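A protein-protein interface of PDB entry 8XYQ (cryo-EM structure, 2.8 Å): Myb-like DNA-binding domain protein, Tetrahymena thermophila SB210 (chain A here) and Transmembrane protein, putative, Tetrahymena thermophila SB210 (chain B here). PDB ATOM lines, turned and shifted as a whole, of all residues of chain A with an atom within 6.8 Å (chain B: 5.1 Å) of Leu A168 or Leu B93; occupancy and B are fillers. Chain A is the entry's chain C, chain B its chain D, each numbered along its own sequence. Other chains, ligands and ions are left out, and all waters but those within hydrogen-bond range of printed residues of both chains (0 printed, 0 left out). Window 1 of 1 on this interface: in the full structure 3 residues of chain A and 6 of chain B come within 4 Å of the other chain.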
ATOM      1  N   PHE A 165       8.612 -23.709   1.577  1.00  0.00           N
ATOM      2  CA  PHE A 165      10.050 -23.782   1.775  1.00  0.00           C
ATOM      3  C   PHE A 165      10.557 -22.525   2.481  1.00  0.00           C
ATOM      4  O   PHE A 165       9.924 -21.467   2.457  1.00  0.00           O
ATOM      5  CB  PHE A 165      10.772 -23.950   0.436  1.00  0.00           C
ATOM      6  CG  PHE A 165      10.787 -25.364  -0.084  1.00  0.00           C
ATOM      7  CD1 PHE A 165       9.620 -26.109  -0.164  1.00  0.00           C
ATOM      8  CD2 PHE A 165      11.972 -25.945  -0.500  1.00  0.00           C
ATOM      9  CE1 PHE A 165       9.637 -27.403  -0.644  1.00  0.00           C
ATOM     10  CE2 PHE A 165      11.995 -27.239  -0.980  1.00  0.00           C
ATOM     11  CZ  PHE A 165      10.826 -27.968  -1.053  1.00  0.00           C
ATOM     12  N   THR A 166      11.719 -22.654   3.115  1.00  0.00           N
ATOM     13  CA  THR A 166      12.385 -21.530   3.758  1.00  0.00           C
ATOM     14  C   THR A 166      13.394 -20.901   2.802  1.00  0.00           C
ATOM     15  O   THR A 166      13.687 -21.429   1.729  1.00  0.00           O
ATOM     16  CB  THR A 166      13.078 -21.968   5.052  1.00  0.00           C
ATOM     17  OG1 THR A 166      14.201 -22.800   4.738  1.00  0.00           O
ATOM     18  CG2 THR A 166      12.111 -22.729   5.947  1.00  0.00           C
ATOM     19  N   ASN A 167      13.938 -19.756   3.217  1.00  0.00           N
ATOM     20  CA  ASN A 167      14.816 -18.970   2.357  1.00  0.00           C
ATOM     21  C   ASN A 167      16.176 -19.617   2.125  1.00  0.00           C
ATOM     22  O   ASN A 167      16.887 -19.194   1.207  1.00  0.00           O
ATOM     23  CB  ASN A 167      15.009 -17.575   2.951  1.00  0.00           C
ATOM     24  CG  ASN A 167      13.717 -16.981   3.470  1.00  0.00           C
ATOM     25  OD1 ASN A 167      12.945 -17.649   4.159  1.00  0.00           O
ATOM     26  ND2 ASN A 167      13.472 -15.719   3.143  1.00  0.00           N
ATOM     27  N   LEU A 168      16.556 -20.617   2.920  1.00  0.00           N
ATOM     28  CA  LEU A 168      17.851 -21.263   2.744  1.00  0.00           C
ATOM     29  C   LEU A 168      17.780 -22.456   1.796  1.00  0.00           C
ATOM     30  O   LEU A 168      18.640 -22.605   0.921  1.00  0.00           O
ATOM     31  CB  LEU A 168      18.411 -21.703   4.097  1.00  0.00           C
ATOM     32  CG  LEU A 168      19.792 -22.354   4.021  1.00  0.00           C
ATOM     33  CD1 LEU A 168      20.812 -21.396   3.423  1.00  0.00           C
ATOM     34  CD2 LEU A 168      20.229 -22.839   5.387  1.00  0.00           C
ATOM     35  N   GLU A 169      16.773 -23.319   1.956  1.00  0.00           N
ATOM     36  CA  GLU A 169      16.617 -24.431   1.024  1.00  0.00           C
ATOM     37  C   GLU A 169      16.247 -23.927  -0.365  1.00  0.00           C
ATOM     38  O   GLU A 169      16.670 -24.504  -1.374  1.00  0.00           O
ATOM     39  CB  GLU A 169      15.571 -25.422   1.533  1.00  0.00           C
ATOM     40  CG  GLU A 169      14.298 -24.798   2.069  1.00  0.00           C
ATOM     41  CD  GLU A 169      13.750 -25.553   3.264  1.00  0.00           C
ATOM     42  OE1 GLU A 169      12.713 -25.129   3.814  1.00  0.00           O
ATOM     43  OE2 GLU A 169      14.360 -26.569   3.656  1.00  0.00           O
ATOM     44  N   ILE A 170      15.472 -22.840  -0.429  1.00  0.00           N
ATOM     45  CA  ILE A 170      15.182 -22.189  -1.705  1.00  0.00           C
ATOM     46  C   ILE A 170      16.476 -21.752  -2.377  1.00  0.00           C
ATOM     47  O   ILE A 170      16.683 -21.984  -3.573  1.00  0.00           O
ATOM     48  CB  ILE A 170      14.227 -20.998  -1.498  1.00  0.00           C
ATOM     49  CG1 ILE A 170      12.784 -21.480  -1.355  1.00  0.00           C
ATOM     50  CG2 ILE A 170      14.335 -20.000  -2.637  1.00  0.00           C
ATOM     51  CD1 ILE A 170      11.791 -20.359  -1.122  1.00  0.00           C
ATOM     52  N   LEU A 171      17.384 -21.156  -1.603  1.00  0.00           N
ATOM     53  CA  LEU A 171      18.606 -20.614  -2.184  1.00  0.00           C
ATOM     54  C   LEU A 171      19.565 -21.732  -2.583  1.00  0.00           C
ATOM     55  O   LEU A 171      20.280 -21.621  -3.588  1.00  0.00           O
ATOM     56  CB  LEU A 171      19.234 -19.626  -1.198  1.00  0.00           C
ATOM     57  CG  LEU A 171      20.066 -18.449  -1.720  1.00  0.00           C
ATOM     58  CD1 LEU A 171      20.223 -17.414  -0.624  1.00  0.00           C
ATOM     59  CD2 LEU A 171      21.422 -18.861  -2.221  1.00  0.00           C
ATOM     60  N   THR A 172      19.557 -22.835  -1.831  1.00  0.00           N
ATOM     61  CA  THR A 172      20.290 -24.030  -2.245  1.00  0.00           C
ATOM     62  C   THR A 172      19.747 -24.571  -3.566  1.00  0.00           C
ATOM     63  O   THR A 172      20.518 -24.969  -4.449  1.00  0.00           O
ATOM     64  CB  THR A 172      20.221 -25.090  -1.140  1.00  0.00           C
ATOM     65  OG1 THR A 172      21.140 -24.754  -0.092  1.00  0.00           O
ATOM     66  CG2 THR A 172      20.568 -26.474  -1.665  1.00  0.00           C
ATOM     67  N   HIS A 173      18.419 -24.564  -3.727  1.00  0.00           N
ATOM     68  CA  HIS A 173      17.816 -24.999  -4.984  1.00  0.00           C
ATOM     69  C   HIS A 173      18.201 -24.080  -6.140  1.00  0.00           C
ATOM     70  O   HIS A 173      18.482 -24.552  -7.249  1.00  0.00           O
ATOM     71  CB  HIS A 173      16.297 -25.070  -4.837  1.00  0.00           C
ATOM     72  CG  HIS A 173      15.832 -26.174  -3.939  1.00  0.00           C
ATOM     73  ND1 HIS A 173      16.563 -27.325  -3.738  1.00  0.00           N
ATOM     74  CD2 HIS A 173      14.719 -26.299  -3.180  1.00  0.00           C
ATOM     75  CE1 HIS A 173      15.917 -28.113  -2.898  1.00  0.00           C
ATOM     76  NE2 HIS A 173      14.796 -27.514  -2.545  1.00  0.00           N
ATOM     77  N   TYR A 175      20.950 -22.311  -6.380  1.00  0.00           N
ATOM     78  CA  TYR A 175      22.356 -22.542  -6.703  1.00  0.00           C
ATOM     79  C   TYR A 175      22.562 -23.870  -7.423  1.00  0.00           C
ATOM     80  O   TYR A 175      23.411 -23.967  -8.315  1.00  0.00           O
ATOM     81  CB  TYR A 175      23.216 -22.475  -5.444  1.00  0.00           C
ATOM     82  CG  TYR A 175      24.020 -21.201  -5.340  1.00  0.00           C
ATOM     83  CD1 TYR A 175      25.031 -20.915  -6.252  1.00  0.00           C
ATOM     84  CD2 TYR A 175      23.773 -20.289  -4.332  1.00  0.00           C
ATOM     85  CE1 TYR A 175      25.770 -19.752  -6.156  1.00  0.00           C
ATOM     86  CE2 TYR A 175      24.501 -19.124  -4.229  1.00  0.00           C
ATOM     87  CZ  TYR A 175      25.498 -18.861  -5.143  1.00  0.00           C
ATOM     88  OH  TYR A 175      26.229 -17.702  -5.047  1.00  0.00           O
ATOM     89  N   GLN B  52      19.170 -26.414  11.237  1.00  0.00           N
ATOM     90  CA  GLN B  52      19.802 -25.324  10.500  1.00  0.00           C
ATOM     91  C   GLN B  52      20.050 -24.110  11.389  1.00  0.00           C
ATOM     92  O   GLN B  52      19.979 -22.971  10.919  1.00  0.00           O
ATOM     93  CB  GLN B  52      18.955 -24.918   9.292  1.00  0.00           C
ATOM     94  CG  GLN B  52      18.775 -25.996   8.238  1.00  0.00           C
ATOM     95  CD  GLN B  52      17.644 -25.687   7.277  1.00  0.00           C
ATOM     96  OE1 GLN B  52      16.957 -26.588   6.799  1.00  0.00           O
ATOM     97  NE2 GLN B  52      17.442 -24.406   6.995  1.00  0.00           N
ATOM     98  N   ASN B  87      26.680 -27.041   5.651  1.00  0.00           N
ATOM     99  CA  ASN B  87      25.871 -26.577   4.529  1.00  0.00           C
ATOM    100  C   ASN B  87      26.681 -25.587   3.701  1.00  0.00           C
ATOM    101  O   ASN B  87      26.850 -24.421   4.078  1.00  0.00           O
ATOM    102  CB  ASN B  87      24.574 -25.951   5.025  1.00  0.00           C
ATOM    103  CG  ASN B  87      23.465 -26.014   3.993  1.00  0.00           C
ATOM    104  OD1 ASN B  87      23.701 -26.338   2.831  1.00  0.00           O
ATOM    105  ND2 ASN B  87      22.244 -25.705   4.415  1.00  0.00           N
ATOM    106  N   VAL B  89      26.850 -23.167   0.439  1.00  0.00           N
ATOM    107  CA  VAL B  89      25.960 -22.061   0.067  1.00  0.00           C
ATOM    108  C   VAL B  89      25.588 -21.284   1.327  1.00  0.00           C
ATOM    109  O   VAL B  89      25.695 -20.055   1.350  1.00  0.00           O
ATOM    110  CB  VAL B  89      24.709 -22.508  -0.722  1.00  0.00           C
ATOM    111  CG1 VAL B  89      23.732 -21.366  -0.875  1.00  0.00           C
ATOM    112  CG2 VAL B  89      25.109 -23.062  -2.080  1.00  0.00           C
ATOM    113  N   GLU B  90      25.179 -21.980   2.392  1.00  0.00           N
ATOM    114  CA  GLU B  90      24.982 -21.298   3.669  1.00  0.00           C
ATOM    115  C   GLU B  90      26.299 -20.779   4.235  1.00  0.00           C
ATOM    116  O   GLU B  90      26.319 -19.713   4.861  1.00  0.00           O
ATOM    117  CB  GLU B  90      24.300 -22.215   4.684  1.00  0.00           C
ATOM    118  CG  GLU B  90      23.945 -21.505   5.989  1.00  0.00           C
ATOM    119  CD  GLU B  90      23.325 -22.418   7.025  1.00  0.00           C
ATOM    120  OE1 GLU B  90      23.778 -23.574   7.151  1.00  0.00           O
ATOM    121  OE2 GLU B  90      22.393 -21.970   7.728  1.00  0.00           O
ATOM    122  N   LEU B  91      27.402 -21.506   4.028  1.00  0.00           N
ATOM    123  CA  LEU B  91      28.707 -20.976   4.425  1.00  0.00           C
ATOM    124  C   LEU B  91      29.034 -19.690   3.672  1.00  0.00           C
ATOM    125  O   LEU B  91      29.549 -18.732   4.260  1.00  0.00           O
ATOM    126  CB  LEU B  91      29.801 -22.019   4.199  1.00  0.00           C
ATOM    127  CG  LEU B  91      29.821 -23.268   5.082  1.00  0.00           C
ATOM    128  CD1 LEU B  91      31.229 -23.827   5.162  1.00  0.00           C
ATOM    129  CD2 LEU B  91      29.286 -22.978   6.470  1.00  0.00           C
ATOM    130  N   GLU B  92      28.724 -19.648   2.373  1.00  0.00           N
ATOM    131  CA  GLU B  92      28.919 -18.429   1.592  1.00  0.00           C
ATOM    132  C   GLU B  92      28.021 -17.300   2.090  1.00  0.00           C
ATOM    133  O   GLU B  92      28.454 -16.144   2.169  1.00  0.00           O
ATOM    134  CB  GLU B  92      28.661 -18.716   0.111  1.00  0.00           C
ATOM    135  CG  GLU B  92      28.169 -17.527  -0.700  1.00  0.00           C
ATOM    136  CD  GLU B  92      28.717 -17.516  -2.111  1.00  0.00           C
ATOM    137  OE1 GLU B  92      28.841 -18.603  -2.712  1.00  0.00           O
ATOM    138  OE2 GLU B  92      29.023 -16.418  -2.622  1.00  0.00           O
ATOM    139  N   LEU B  93      26.774 -17.623   2.440  1.00  0.00           N
ATOM    140  CA  LEU B  93      25.842 -16.626   2.966  1.00  0.00           C
ATOM    141  C   LEU B  93      26.354 -16.024   4.269  1.00  0.00           C
ATOM    142  O   LEU B  93      26.329 -14.802   4.461  1.00  0.00           O
ATOM    143  CB  LEU B  93      24.471 -17.269   3.186  1.00  0.00           C
ATOM    144  CG  LEU B  93      23.636 -17.688   1.975  1.00  0.00           C
ATOM    145  CD1 LEU B  93      22.214 -17.989   2.387  1.00  0.00           C
ATOM    146  CD2 LEU B  93      23.656 -16.615   0.914  1.00  0.00           C
ATOM    147  N   ARG B  94      26.839 -16.875   5.175  1.00  0.00           N
ATOM    148  CA  ARG B  94      27.317 -16.384   6.463  1.00  0.00           C
ATOM    149  C   ARG B  94      28.620 -15.606   6.312  1.00  0.00           C
ATOM    150  O   ARG B  94      28.832 -14.608   7.011  1.00  0.00           O
ATOM    151  CB  ARG B  94      27.479 -17.546   7.441  1.00  0.00           C
ATOM    152  CG  ARG B  94      26.184 -18.297   7.710  1.00  0.00           C
ATOM    153  CD  ARG B  94      25.410 -17.702   8.869  1.00  0.00           C
ATOM    154  NE  ARG B  94      24.151 -18.404   9.089  1.00  0.00           N
ATOM    155  CZ  ARG B  94      23.157 -17.942   9.832  1.00  0.00           C
ATOM    156  NH1 ARG B  94      23.239 -16.775  10.448  1.00  0.00           N
ATOM    157  NH2 ARG B  94      22.052 -18.671   9.965  1.00  0.00           N
ATOM    158  N   THR B  95      29.497 -16.033   5.397  1.00  0.00           N
ATOM    159  CA  THR B  95      30.705 -15.257   5.134  1.00  0.00           C
ATOM    160  C   THR B  95      30.380 -13.910   4.499  1.00  0.00           C
ATOM    161  O   THR B  95      31.082 -12.924   4.750  1.00  0.00           O
ATOM    162  CB  THR B  95      31.661 -16.049   4.244  1.00  0.00           C
ATOM    163  OG1 THR B  95      31.682 -17.417   4.668  1.00  0.00           O
ATOM    164  CG2 THR B  95      33.068 -15.478   4.338  1.00  0.00           C
ATOM    165  N   CYS B  96      29.331 -13.848   3.673  1.00  0.00           N
ATOM    166  CA  CYS B  96      28.845 -12.561   3.183  1.00  0.00           C
ATOM    167  C   CYS B  96      28.343 -11.694   4.328  1.00  0.00           C
ATOM    168  O   CYS B  96      28.588 -10.483   4.358  1.00  0.00           O
ATOM    169  CB  CYS B  96      27.728 -12.769   2.160  1.00  0.00           C
ATOM    170  SG  CYS B  96      28.262 -13.164   0.486  1.00  0.00           S
ATOM    171  N   MET B  97      27.629 -12.301   5.279  1.00  0.00           N
ATOM    172  CA  MET B  97      27.036 -11.524   6.363  1.00  0.00           C
ATOM    173  C   MET B  97      28.076 -11.047   7.372  1.00  0.00           C
ATOM    174  O   MET B  97      27.853 -10.034   8.045  1.00  0.00           O
ATOM    175  CB  MET B  97      25.956 -12.336   7.070  1.00  0.00           C
ATOM    176  CG  MET B  97      24.849 -11.475   7.645  1.00  0.00           C
ATOM    177  SD  MET B  97      23.526 -12.417   8.419  1.00  0.00           S
ATOM    178  CE  MET B  97      22.923 -11.213   9.600  1.00  0.00           C
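O of Glu B92 is in hydrogen-bond range of SG of Cys B96.
The side-chain hydroxyl of Thr A172 lies within hydrogen-bond range of the backbone carbonyl oxygen of Leu A168 (3.4 Å).
Among the printed residues, pairs that only touch across the chains: Leu A168 with Glu B90 (3.3 Å), Leu A168 with Gln B52 (3.6 Å), Tyr A175 with Glu B92 (3.6 Å), Tyr A175 with Val B89 (3.6 Å), Leu A168 with Asn B87 (3.6 Å), Leu A171 with Leu B93 (3.7 Å), Leu A171 with Val B89 (3.7 Å) and Leu A168 with Leu B93 (3.8 Å).
Of the printed residues of chain B, Leu A168 touches Gln B52, Asn B87, Glu B90 and Leu B93.
Of chain A, only Leu A168 (3.8 Å) and Leu A171 (3.7 Å) come within 4 Å of Leu B93.
Of the printed residues of chain A, Glu B92 touches Tyr A175.
Of the printed residues of chain B, Leu A171 touches Val B89 and Leu B93.
Thr B95 touches none of the printed residues of chain A.
His A173 touches none of the printed residues of chain B.
The nearest residue of chain A that does not touch Leu B93 is Asn A167 (5.6 Å).
The nearest printed residue of chain A that does not touch Gln B52 is Glu A169 (4.1 Å).
Hydrophobic or aromatic side chains of chain B that line the printed part of chain A: Val B89 and Leu B93.
Among the printed residues, no Asp or Glu carboxylate lies within 4 Å of a Lys or Arg side-chain nitrogen of the other chain.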
